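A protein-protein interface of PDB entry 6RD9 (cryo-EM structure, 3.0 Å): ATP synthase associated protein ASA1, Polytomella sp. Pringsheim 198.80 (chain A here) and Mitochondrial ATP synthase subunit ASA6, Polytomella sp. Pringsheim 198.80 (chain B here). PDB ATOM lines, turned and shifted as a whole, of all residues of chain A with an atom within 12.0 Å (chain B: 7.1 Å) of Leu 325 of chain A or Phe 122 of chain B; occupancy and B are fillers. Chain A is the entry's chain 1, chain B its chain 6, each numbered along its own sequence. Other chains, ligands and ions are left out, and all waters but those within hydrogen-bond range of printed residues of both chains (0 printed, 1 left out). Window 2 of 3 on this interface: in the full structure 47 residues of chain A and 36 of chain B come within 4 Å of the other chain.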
ATOM      1  N   LEU A 315     -26.115   9.640 -20.320  1.00  0.00           N
ATOM      2  CA  LEU A 315     -26.397   8.466 -19.515  1.00  0.00           C
ATOM      3  C   LEU A 315     -25.540   7.279 -19.887  1.00  0.00           C
ATOM      4  O   LEU A 315     -25.346   6.403 -19.061  1.00  0.00           O
ATOM      5  CB  LEU A 315     -27.850   8.051 -19.656  1.00  0.00           C
ATOM      6  CG  LEU A 315     -28.856   8.513 -18.626  1.00  0.00           C
ATOM      7  CD1 LEU A 315     -30.143   7.862 -18.948  1.00  0.00           C
ATOM      8  CD2 LEU A 315     -28.422   8.115 -17.265  1.00  0.00           C
ATOM      9  N   ASN A 316     -25.057   7.199 -21.115  1.00  0.00           N
ATOM     10  CA  ASN A 316     -24.253   6.056 -21.511  1.00  0.00           C
ATOM     11  C   ASN A 316     -22.877   6.098 -20.893  1.00  0.00           C
ATOM     12  O   ASN A 316     -22.261   5.053 -20.684  1.00  0.00           O
ATOM     13  CB  ASN A 316     -24.122   6.022 -23.012  1.00  0.00           C
ATOM     14  CG  ASN A 316     -25.271   5.382 -23.649  1.00  0.00           C
ATOM     15  OD1 ASN A 316     -25.800   5.861 -24.637  1.00  0.00           O
ATOM     16  ND2 ASN A 316     -25.678   4.271 -23.098  1.00  0.00           N
ATOM     17  N   SER A 318     -22.464   7.423 -17.940  1.00  0.00           N
ATOM     18  CA  SER A 318     -22.729   7.444 -16.518  1.00  0.00           C
ATOM     19  C   SER A 318     -22.030   6.270 -15.855  1.00  0.00           C
ATOM     20  O   SER A 318     -21.682   5.297 -16.523  1.00  0.00           O
ATOM     21  CB  SER A 318     -24.227   7.352 -16.280  1.00  0.00           C
ATOM     22  OG  SER A 318     -24.598   7.684 -14.968  1.00  0.00           O
ATOM     23  N   PRO A 319     -21.814   6.325 -14.540  1.00  0.00           N
ATOM     24  CA  PRO A 319     -21.324   5.135 -13.841  1.00  0.00           C
ATOM     25  C   PRO A 319     -22.301   3.985 -13.823  1.00  0.00           C
ATOM     26  O   PRO A 319     -21.903   2.869 -13.501  1.00  0.00           O
ATOM     27  CB  PRO A 319     -21.057   5.655 -12.433  1.00  0.00           C
ATOM     28  CG  PRO A 319     -20.800   7.048 -12.605  1.00  0.00           C
ATOM     29  CD  PRO A 319     -21.639   7.524 -13.712  1.00  0.00           C
ATOM     30  N   ALA A 320     -23.565   4.213 -14.148  1.00  0.00           N
ATOM     31  CA  ALA A 320     -24.542   3.142 -14.120  1.00  0.00           C
ATOM     32  C   ALA A 320     -24.378   2.191 -15.274  1.00  0.00           C
ATOM     33  O   ALA A 320     -24.731   1.022 -15.155  1.00  0.00           O
ATOM     34  CB  ALA A 320     -25.939   3.717 -14.159  1.00  0.00           C
ATOM     35  N   PHE A 321     -23.892   2.668 -16.404  1.00  0.00           N
ATOM     36  CA  PHE A 321     -23.861   1.872 -17.614  1.00  0.00           C
ATOM     37  C   PHE A 321     -22.517   1.220 -17.835  1.00  0.00           C
ATOM     38  O   PHE A 321     -22.356   0.459 -18.781  1.00  0.00           O
ATOM     39  CB  PHE A 321     -24.257   2.728 -18.805  1.00  0.00           C
ATOM     40  CG  PHE A 321     -25.723   2.842 -18.973  1.00  0.00           C
ATOM     41  CD1 PHE A 321     -26.380   2.106 -19.916  1.00  0.00           C
ATOM     42  CD2 PHE A 321     -26.450   3.647 -18.153  1.00  0.00           C
ATOM     43  CE1 PHE A 321     -27.730   2.190 -20.038  1.00  0.00           C
ATOM     44  CE2 PHE A 321     -27.786   3.737 -18.283  1.00  0.00           C
ATOM     45  CZ  PHE A 321     -28.426   3.002 -19.223  1.00  0.00           C
ATOM     46  N   SER A 322     -21.554   1.507 -16.988  1.00  0.00           N
ATOM     47  CA  SER A 322     -20.341   0.728 -16.903  1.00  0.00           C
ATOM     48  C   SER A 322     -20.459  -0.384 -15.883  1.00  0.00           C
ATOM     49  O   SER A 322     -19.479  -1.087 -15.641  1.00  0.00           O
ATOM     50  CB  SER A 322     -19.168   1.616 -16.533  1.00  0.00           C
ATOM     51  OG  SER A 322     -19.287   2.029 -15.189  1.00  0.00           O
ATOM     52  N   SER A 323     -21.614  -0.529 -15.249  1.00  0.00           N
ATOM     53  CA  SER A 323     -21.849  -1.642 -14.356  1.00  0.00           C
ATOM     54  C   SER A 323     -22.031  -2.907 -15.162  1.00  0.00           C
ATOM     55  O   SER A 323     -22.251  -2.869 -16.368  1.00  0.00           O
ATOM     56  CB  SER A 323     -23.070  -1.393 -13.494  1.00  0.00           C
ATOM     57  OG  SER A 323     -22.820  -0.343 -12.596  1.00  0.00           O
ATOM     58  N   PHE A 324     -21.966  -4.040 -14.469  1.00  0.00           N
ATOM     59  CA  PHE A 324     -21.907  -5.324 -15.146  1.00  0.00           C
ATOM     60  C   PHE A 324     -23.208  -5.645 -15.860  1.00  0.00           C
ATOM     61  O   PHE A 324     -23.196  -6.097 -17.002  1.00  0.00           O
ATOM     62  CB  PHE A 324     -21.568  -6.425 -14.153  1.00  0.00           C
ATOM     63  CG  PHE A 324     -21.444  -7.766 -14.786  1.00  0.00           C
ATOM     64  CD1 PHE A 324     -20.322  -8.087 -15.507  1.00  0.00           C
ATOM     65  CD2 PHE A 324     -22.460  -8.690 -14.694  1.00  0.00           C
ATOM     66  CE1 PHE A 324     -20.216  -9.290 -16.104  1.00  0.00           C
ATOM     67  CE2 PHE A 324     -22.350  -9.884 -15.302  1.00  0.00           C
ATOM     68  CZ  PHE A 324     -21.230 -10.183 -16.006  1.00  0.00           C
ATOM     69  N   LEU A 325     -24.334  -5.428 -15.212  1.00  0.00           N
ATOM     70  CA  LEU A 325     -25.604  -5.798 -15.813  1.00  0.00           C
ATOM     71  C   LEU A 325     -26.084  -4.806 -16.851  1.00  0.00           C
ATOM     72  O   LEU A 325     -27.070  -5.083 -17.535  1.00  0.00           O
ATOM     73  CB  LEU A 325     -26.659  -5.940 -14.734  1.00  0.00           C
ATOM     74  CG  LEU A 325     -26.352  -7.037 -13.738  1.00  0.00           C
ATOM     75  CD1 LEU A 325     -27.247  -6.880 -12.562  1.00  0.00           C
ATOM     76  CD2 LEU A 325     -26.579  -8.364 -14.397  1.00  0.00           C
ATOM     77  N   LEU A 326     -25.436  -3.656 -16.972  1.00  0.00           N
ATOM     78  CA  LEU A 326     -25.825  -2.651 -17.945  1.00  0.00           C
ATOM     79  C   LEU A 326     -24.704  -2.345 -18.911  1.00  0.00           C
ATOM     80  O   LEU A 326     -24.738  -1.312 -19.570  1.00  0.00           O
ATOM     81  CB  LEU A 326     -26.257  -1.366 -17.249  1.00  0.00           C
ATOM     82  CG  LEU A 326     -27.584  -1.345 -16.523  1.00  0.00           C
ATOM     83  CD1 LEU A 326     -27.765  -0.001 -15.962  1.00  0.00           C
ATOM     84  CD2 LEU A 326     -28.659  -1.638 -17.492  1.00  0.00           C
ATOM     85  N   LYS A 327     -23.720  -3.234 -19.021  1.00  0.00           N
ATOM     86  CA  LYS A 327     -22.498  -2.908 -19.743  1.00  0.00           C
ATOM     87  C   LYS A 327     -22.712  -2.907 -21.248  1.00  0.00           C
ATOM     88  O   LYS A 327     -22.177  -2.049 -21.952  1.00  0.00           O
ATOM     89  CB  LYS A 327     -21.399  -3.883 -19.366  1.00  0.00           C
ATOM     90  CG  LYS A 327     -20.045  -3.302 -19.494  1.00  0.00           C
ATOM     91  CD  LYS A 327     -19.008  -4.204 -18.900  1.00  0.00           C
ATOM     92  CE  LYS A 327     -19.083  -4.194 -17.416  1.00  0.00           C
ATOM     93  NZ  LYS A 327     -18.011  -4.991 -16.798  1.00  0.00           N
ATOM     94  N   ARG A 328     -23.517  -3.860 -21.726  1.00  0.00           N
ATOM     95  CA  ARG A 328     -23.811  -3.982 -23.180  1.00  0.00           C
ATOM     96  C   ARG A 328     -25.146  -3.298 -23.497  1.00  0.00           C
ATOM     97  O   ARG A 328     -25.762  -3.660 -24.519  1.00  0.00           O
ATOM     98  CB  ARG A 328     -23.834  -5.456 -23.597  1.00  0.00           C
ATOM     99  CG  ARG A 328     -22.486  -6.154 -23.490  1.00  0.00           C
ATOM    100  CD  ARG A 328     -22.537  -7.589 -23.981  1.00  0.00           C
ATOM    101  NE  ARG A 328     -21.253  -8.262 -23.856  1.00  0.00           N
ATOM    102  CZ  ARG A 328     -20.264  -8.168 -24.739  1.00  0.00           C
ATOM    103  NH1 ARG A 328     -20.412  -7.422 -25.821  1.00  0.00           N
ATOM    104  NH2 ARG A 328     -19.134  -8.819 -24.538  1.00  0.00           N
ATOM    105  N   GLU A 329     -25.574  -2.351 -22.655  1.00  0.00           N
ATOM    106  CA  GLU A 329     -26.824  -1.653 -22.891  1.00  0.00           C
ATOM    107  C   GLU A 329     -26.570  -0.232 -23.357  1.00  0.00           C
ATOM    108  O   GLU A 329     -25.505   0.344 -23.138  1.00  0.00           O
ATOM    109  CB  GLU A 329     -27.679  -1.630 -21.632  1.00  0.00           C
ATOM    110  CG  GLU A 329     -28.397  -2.910 -21.366  1.00  0.00           C
ATOM    111  CD  GLU A 329     -29.156  -3.396 -22.565  1.00  0.00           C
ATOM    112  OE1 GLU A 329     -28.965  -4.567 -22.943  1.00  0.00           O
ATOM    113  OE2 GLU A 329     -29.943  -2.614 -23.139  1.00  0.00           O
ATOM    114  N   LYS A 330     -27.575   0.330 -24.001  1.00  0.00           N
ATOM    115  CA  LYS A 330     -27.517   1.695 -24.473  1.00  0.00           C
ATOM    116  C   LYS A 330     -28.750   2.428 -23.984  1.00  0.00           C
ATOM    117  O   LYS A 330     -29.851   1.883 -24.010  1.00  0.00           O
ATOM    118  CB  LYS A 330     -27.422   1.743 -25.991  1.00  0.00           C
ATOM    119  CG  LYS A 330     -26.081   1.291 -26.524  1.00  0.00           C
ATOM    120  CD  LYS A 330     -24.967   2.108 -25.914  1.00  0.00           C
ATOM    121  CE  LYS A 330     -23.661   1.354 -25.901  1.00  0.00           C
ATOM    122  NZ  LYS A 330     -22.609   2.150 -25.210  1.00  0.00           N
ATOM    123  N   ALA A 331     -28.558   3.663 -23.535  1.00  0.00           N
ATOM    124  CA  ALA A 331     -29.654   4.448 -23.000  1.00  0.00           C
ATOM    125  C   ALA A 331     -30.606   4.919 -24.079  1.00  0.00           C
ATOM    126  O   ALA A 331     -31.758   5.231 -23.774  1.00  0.00           O
ATOM    127  CB  ALA A 331     -29.110   5.649 -22.247  1.00  0.00           C
ATOM    128  N   GLU A 332     -30.153   4.976 -25.329  1.00  0.00           N
ATOM    129  CA  GLU A 332     -31.015   5.361 -26.436  1.00  0.00           C
ATOM    130  C   GLU A 332     -32.000   4.269 -26.789  1.00  0.00           C
ATOM    131  O   GLU A 332     -32.965   4.530 -27.508  1.00  0.00           O
ATOM    132  CB  GLU A 332     -30.177   5.687 -27.664  1.00  0.00           C
ATOM    133  CG  GLU A 332     -29.115   6.740 -27.454  1.00  0.00           C
ATOM    134  CD  GLU A 332     -27.779   6.154 -27.066  1.00  0.00           C
ATOM    135  OE1 GLU A 332     -27.757   5.015 -26.572  1.00  0.00           O
ATOM    136  OE2 GLU A 332     -26.748   6.827 -27.255  1.00  0.00           O
ATOM    137  N   SER A 333     -31.763   3.048 -26.318  1.00  0.00           N
ATOM    138  CA  SER A 333     -32.674   1.944 -26.563  1.00  0.00           C
ATOM    139  C   SER A 333     -33.950   2.066 -25.757  1.00  0.00           C
ATOM    140  O   SER A 333     -34.935   1.401 -26.083  1.00  0.00           O
ATOM    141  CB  SER A 333     -31.984   0.629 -26.237  1.00  0.00           C
ATOM    142  OG  SER A 333     -30.855   0.448 -27.062  1.00  0.00           O
ATOM    143  N   GLU A 334     -33.958   2.873 -24.703  1.00  0.00           N
ATOM    144  CA  GLU A 334     -35.166   3.006 -23.907  1.00  0.00           C
ATOM    145  C   GLU A 334     -36.061   4.101 -24.455  1.00  0.00           C
ATOM    146  O   GLU A 334     -37.171   3.830 -24.921  1.00  0.00           O
ATOM    147  CB  GLU A 334     -34.817   3.280 -22.448  1.00  0.00           C
ATOM    148  CG  GLU A 334     -36.035   3.419 -21.563  1.00  0.00           C
ATOM    149  CD  GLU A 334     -36.560   2.089 -21.057  1.00  0.00           C
ATOM    150  OE1 GLU A 334     -35.998   1.042 -21.428  1.00  0.00           O
ATOM    151  OE2 GLU A 334     -37.532   2.097 -20.274  1.00  0.00           O
ATOM    152  N   PHE B 116     -32.567 -15.549 -13.086  1.00  0.00           N
ATOM    153  CA  PHE B 116     -32.864 -14.131 -12.969  1.00  0.00           C
ATOM    154  C   PHE B 116     -31.848 -13.283 -13.702  1.00  0.00           C
ATOM    155  O   PHE B 116     -32.178 -12.186 -14.145  1.00  0.00           O
ATOM    156  CB  PHE B 116     -32.922 -13.731 -11.506  1.00  0.00           C
ATOM    157  CG  PHE B 116     -34.226 -14.029 -10.861  1.00  0.00           C
ATOM    158  CD1 PHE B 116     -35.366 -14.159 -11.612  1.00  0.00           C
ATOM    159  CD2 PHE B 116     -34.311 -14.188  -9.501  1.00  0.00           C
ATOM    160  CE1 PHE B 116     -36.565 -14.429 -11.012  1.00  0.00           C
ATOM    161  CE2 PHE B 116     -35.501 -14.469  -8.911  1.00  0.00           C
ATOM    162  CZ  PHE B 116     -36.630 -14.583  -9.664  1.00  0.00           C
ATOM    163  N   SER B 117     -30.625 -13.770 -13.868  1.00  0.00           N
ATOM    164  CA  SER B 117     -29.664 -13.070 -14.701  1.00  0.00           C
ATOM    165  C   SER B 117     -29.988 -13.186 -16.175  1.00  0.00           C
ATOM    166  O   SER B 117     -29.430 -12.443 -16.979  1.00  0.00           O
ATOM    167  CB  SER B 117     -28.271 -13.618 -14.466  1.00  0.00           C
ATOM    168  OG  SER B 117     -27.998 -13.680 -13.089  1.00  0.00           O
ATOM    169  N   SER B 118     -30.859 -14.107 -16.549  1.00  0.00           N
ATOM    170  CA  SER B 118     -31.162 -14.367 -17.936  1.00  0.00           C
ATOM    171  C   SER B 118     -32.575 -13.991 -18.318  1.00  0.00           C
ATOM    172  O   SER B 118     -32.961 -14.204 -19.467  1.00  0.00           O
ATOM    173  CB  SER B 118     -30.936 -15.846 -18.249  1.00  0.00           C
ATOM    174  OG  SER B 118     -29.565 -16.101 -18.494  1.00  0.00           O
ATOM    175  N   LEU B 119     -33.358 -13.445 -17.402  1.00  0.00           N
ATOM    176  CA  LEU B 119     -34.740 -13.143 -17.719  1.00  0.00           C
ATOM    177  C   LEU B 119     -35.135 -11.731 -17.339  1.00  0.00           C
ATOM    178  O   LEU B 119     -36.080 -11.183 -17.908  1.00  0.00           O
ATOM    179  CB  LEU B 119     -35.665 -14.126 -17.024  1.00  0.00           C
ATOM    180  CG  LEU B 119     -35.731 -15.483 -17.690  1.00  0.00           C
ATOM    181  CD1 LEU B 119     -36.595 -16.396 -16.868  1.00  0.00           C
ATOM    182  CD2 LEU B 119     -36.282 -15.327 -19.082  1.00  0.00           C
ATOM    183  N   ILE B 120     -34.460 -11.145 -16.365  1.00  0.00           N
ATOM    184  CA  ILE B 120     -34.832  -9.796 -15.947  1.00  0.00           C
ATOM    185  C   ILE B 120     -34.333  -8.806 -16.989  1.00  0.00           C
ATOM    186  O   ILE B 120     -33.150  -8.850 -17.354  1.00  0.00           O
ATOM    187  CB  ILE B 120     -34.249  -9.486 -14.579  1.00  0.00           C
ATOM    188  CG1 ILE B 120     -34.870 -10.382 -13.527  1.00  0.00           C
ATOM    189  CG2 ILE B 120     -34.538  -8.070 -14.205  1.00  0.00           C
ATOM    190  CD1 ILE B 120     -34.269 -10.207 -12.172  1.00  0.00           C
ATOM    191  N   PRO B 121     -35.179  -7.948 -17.530  1.00  0.00           N
ATOM    192  CA  PRO B 121     -34.673  -6.917 -18.433  1.00  0.00           C
ATOM    193  C   PRO B 121     -33.981  -5.828 -17.646  1.00  0.00           C
ATOM    194  O   PRO B 121     -34.631  -4.949 -17.087  1.00  0.00           O
ATOM    195  CB  PRO B 121     -35.935  -6.418 -19.130  1.00  0.00           C
ATOM    196  CG  PRO B 121     -37.041  -6.746 -18.211  1.00  0.00           C
ATOM    197  CD  PRO B 121     -36.642  -7.913 -17.398  1.00  0.00           C
ATOM    198  N   PHE B 122     -32.657  -5.848 -17.614  1.00  0.00           N
ATOM    199  CA  PHE B 122     -31.950  -5.006 -16.671  1.00  0.00           C
ATOM    200  C   PHE B 122     -31.872  -3.561 -17.106  1.00  0.00           C
ATOM    201  O   PHE B 122     -31.608  -2.699 -16.274  1.00  0.00           O
ATOM    202  CB  PHE B 122     -30.554  -5.542 -16.445  1.00  0.00           C
ATOM    203  CG  PHE B 122     -30.515  -6.734 -15.582  1.00  0.00           C
ATOM    204  CD1 PHE B 122     -30.778  -6.630 -14.242  1.00  0.00           C
ATOM    205  CD2 PHE B 122     -30.207  -7.964 -16.105  1.00  0.00           C
ATOM    206  CE1 PHE B 122     -30.733  -7.728 -13.441  1.00  0.00           C
ATOM    207  CE2 PHE B 122     -30.156  -9.059 -15.305  1.00  0.00           C
ATOM    208  CZ  PHE B 122     -30.420  -8.940 -13.973  1.00  0.00           C
ATOM    209  N   ARG B 123     -32.072  -3.275 -18.379  1.00  0.00           N
ATOM    210  CA  ARG B 123     -32.162  -1.892 -18.795  1.00  0.00           C
ATOM    211  C   ARG B 123     -33.558  -1.357 -18.595  1.00  0.00           C
ATOM    212  O   ARG B 123     -33.730  -0.170 -18.340  1.00  0.00           O
ATOM    213  CB  ARG B 123     -31.752  -1.748 -20.247  1.00  0.00           C
ATOM    214  CG  ARG B 123     -31.428  -0.347 -20.663  1.00  0.00           C
ATOM    215  CD  ARG B 123     -31.880  -0.099 -22.066  1.00  0.00           C
ATOM    216  NE  ARG B 123     -33.273  -0.466 -22.245  1.00  0.00           N
ATOM    217  CZ  ARG B 123     -33.696  -1.354 -23.131  1.00  0.00           C
ATOM    218  NH1 ARG B 123     -32.828  -1.966 -23.912  1.00  0.00           N
ATOM    219  NH2 ARG B 123     -34.982  -1.634 -23.229  1.00  0.00           N
ATOM    220  N   ALA B 124     -34.562  -2.205 -18.711  1.00  0.00           N
ATOM    221  CA  ALA B 124     -35.911  -1.759 -18.442  1.00  0.00           C
ATOM    222  C   ALA B 124     -36.157  -1.610 -16.962  1.00  0.00           C
ATOM    223  O   ALA B 124     -36.956  -0.770 -16.563  1.00  0.00           O
ATOM    224  CB  ALA B 124     -36.915  -2.728 -19.037  1.00  0.00           C
ATOM    225  N   VAL B 125     -35.487  -2.414 -16.142  1.00  0.00           N
ATOM    226  CA  VAL B 125     -35.590  -2.299 -14.693  1.00  0.00           C
ATOM    227  C   VAL B 125     -34.877  -1.051 -14.203  1.00  0.00           C
ATOM    228  O   VAL B 125     -35.355  -0.374 -13.292  1.00  0.00           O
ATOM    229  CB  VAL B 125     -35.047  -3.585 -14.049  1.00  0.00           C
ATOM    230  CG1 VAL B 125     -34.692  -3.407 -12.621  1.00  0.00           C
ATOM    231  CG2 VAL B 125     -36.081  -4.646 -14.140  1.00  0.00           C
ATOM    232  N   TYR B 126     -33.750  -0.705 -14.823  1.00  0.00           N
ATOM    233  CA  TYR B 126     -33.014   0.497 -14.451  1.00  0.00           C
ATOM    234  C   TYR B 126     -33.824   1.743 -14.737  1.00  0.00           C
ATOM    235  O   TYR B 126     -33.846   2.676 -13.937  1.00  0.00           O
ATOM    236  CB  TYR B 126     -31.692   0.555 -15.200  1.00  0.00           C
ATOM    237  CG  TYR B 126     -30.919   1.813 -14.953  1.00  0.00           C
ATOM    238  CD1 TYR B 126     -30.209   1.982 -13.790  1.00  0.00           C
ATOM    239  CD2 TYR B 126     -30.894   2.831 -15.880  1.00  0.00           C
ATOM    240  CE1 TYR B 126     -29.520   3.122 -13.554  1.00  0.00           C
ATOM    241  CE2 TYR B 126     -30.214   3.973 -15.644  1.00  0.00           C
ATOM    242  CZ  TYR B 126     -29.527   4.108 -14.482  1.00  0.00           C
ATOM    243  OH  TYR B 126     -28.835   5.251 -14.244  1.00  0.00           O
ATOM    244  N   PHE B 127     -34.491   1.786 -15.873  1.00  0.00           N
ATOM    245  CA  PHE B 127     -35.288   2.949 -16.209  1.00  0.00           C
ATOM    246  C   PHE B 127     -36.648   2.922 -15.557  1.00  0.00           C
ATOM    247  O   PHE B 127     -37.348   3.931 -15.595  1.00  0.00           O
ATOM    248  CB  PHE B 127     -35.441   3.060 -17.716  1.00  0.00           C
ATOM    249  CG  PHE B 127     -34.272   3.678 -18.385  1.00  0.00           C
ATOM    250  CD1 PHE B 127     -34.119   5.035 -18.396  1.00  0.00           C
ATOM    251  CD2 PHE B 127     -33.317   2.904 -18.987  1.00  0.00           C
ATOM    252  CE1 PHE B 127     -33.037   5.600 -18.993  1.00  0.00           C
ATOM    253  CE2 PHE B 127     -32.243   3.467 -19.583  1.00  0.00           C
ATOM    254  CZ  PHE B 127     -32.103   4.810 -19.587  1.00  0.00           C
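Among the printed residues, merely in contact across the chains: Leu 315 of chain A with Phe 127 of chain B, Ala 320 of chain A with Tyr 126 of chain B, Phe 321 of chain A with Tyr 126 of chain B, Phe 321 of chain A with Phe 127 of chain B, Leu 325 of chain A with Phe 122 of chain B, Leu 326 of chain A with Phe 122 of chain B, Leu 326 of chain A with Arg 123 of chain B, Leu 326 of chain A with Tyr 126 of chain B, Lys 330 of chain A with Arg 123 of chain B, Ser 333 of chain A with Arg 123 of chain B and Glu 334 of chain A with Phe 127 of chain B.
The backbone carbonyl oxygen of Ala 320 of chain A sits close to the side-chain hydroxyl of Ser 323 of chain A, at 3.5 Å.
Of chain B, only Phe 122 comes within 4 Å of Leu 325 of chain A. Of the printed residues of chain B, Leu 326 of chain A touches Phe 122, Arg 123 and Tyr 126. No residue of chain A comes within 4 Å of Ser 117 of chain B. No residue of chain A comes within 4 Å of Ser 118 of chain B. Ile 120 of chain B touches none of the printed residues of chain A. No residue of chain A comes within 4 Å of Pro 121 of chain B. Phe 122 of chain B touches just these residues of chain A: Leu 325 and Leu 326. No residue of chain A comes within 4 Å of Ala 124 of chain B. Val 125 of chain B touches none of the printed residues of chain A. Of the printed residues of chain A, Tyr 126 of chain B touches Ala 320, Phe 321 and Leu 326. Printed residues of chain A within 4 Å of Phe 127 of chain B: Leu 315 (3.7 Å), Phe 321 (3.9 Å) and Glu 334 (3.4 Å). The nearest residue of chain B that does not touch Leu 325 of chain A is Arg 123 of chain B (5.4 Å). The nearest residue of chain A that does not touch Phe 122 of chain B is Glu 329 of chain A (5.5 Å). The nearest printed residue of chain B that does not touch Ser 333 of chain A is Phe 127 of chain B (6.6 Å).
Printed residues of chain B that touch a printed residue of chain A: Phe 122, Arg 123, Tyr 126 and Phe 127. Hydrophobic or aromatic side chains of chain B within 4 Å of the printed part of chain A: Phe 122, Tyr 126 and Phe 127. Among the printed residues, Asp or Glu carboxylates within 4 Å of a Lys or Arg side-chain nitrogen of the other chain: Glu 329 of chain A with Arg 123 of chain B and Glu 334 of chain A with Arg 123 of chain B.
OE2 of Glu 329 of chain A is in salt-bridge range of NH1 of Arg 123 of chain B. The side-chain carboxylate (OE1) of Glu 334 of chain A is in salt-bridge range of the guanidinium group (NE) of Arg 123 of chain B.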
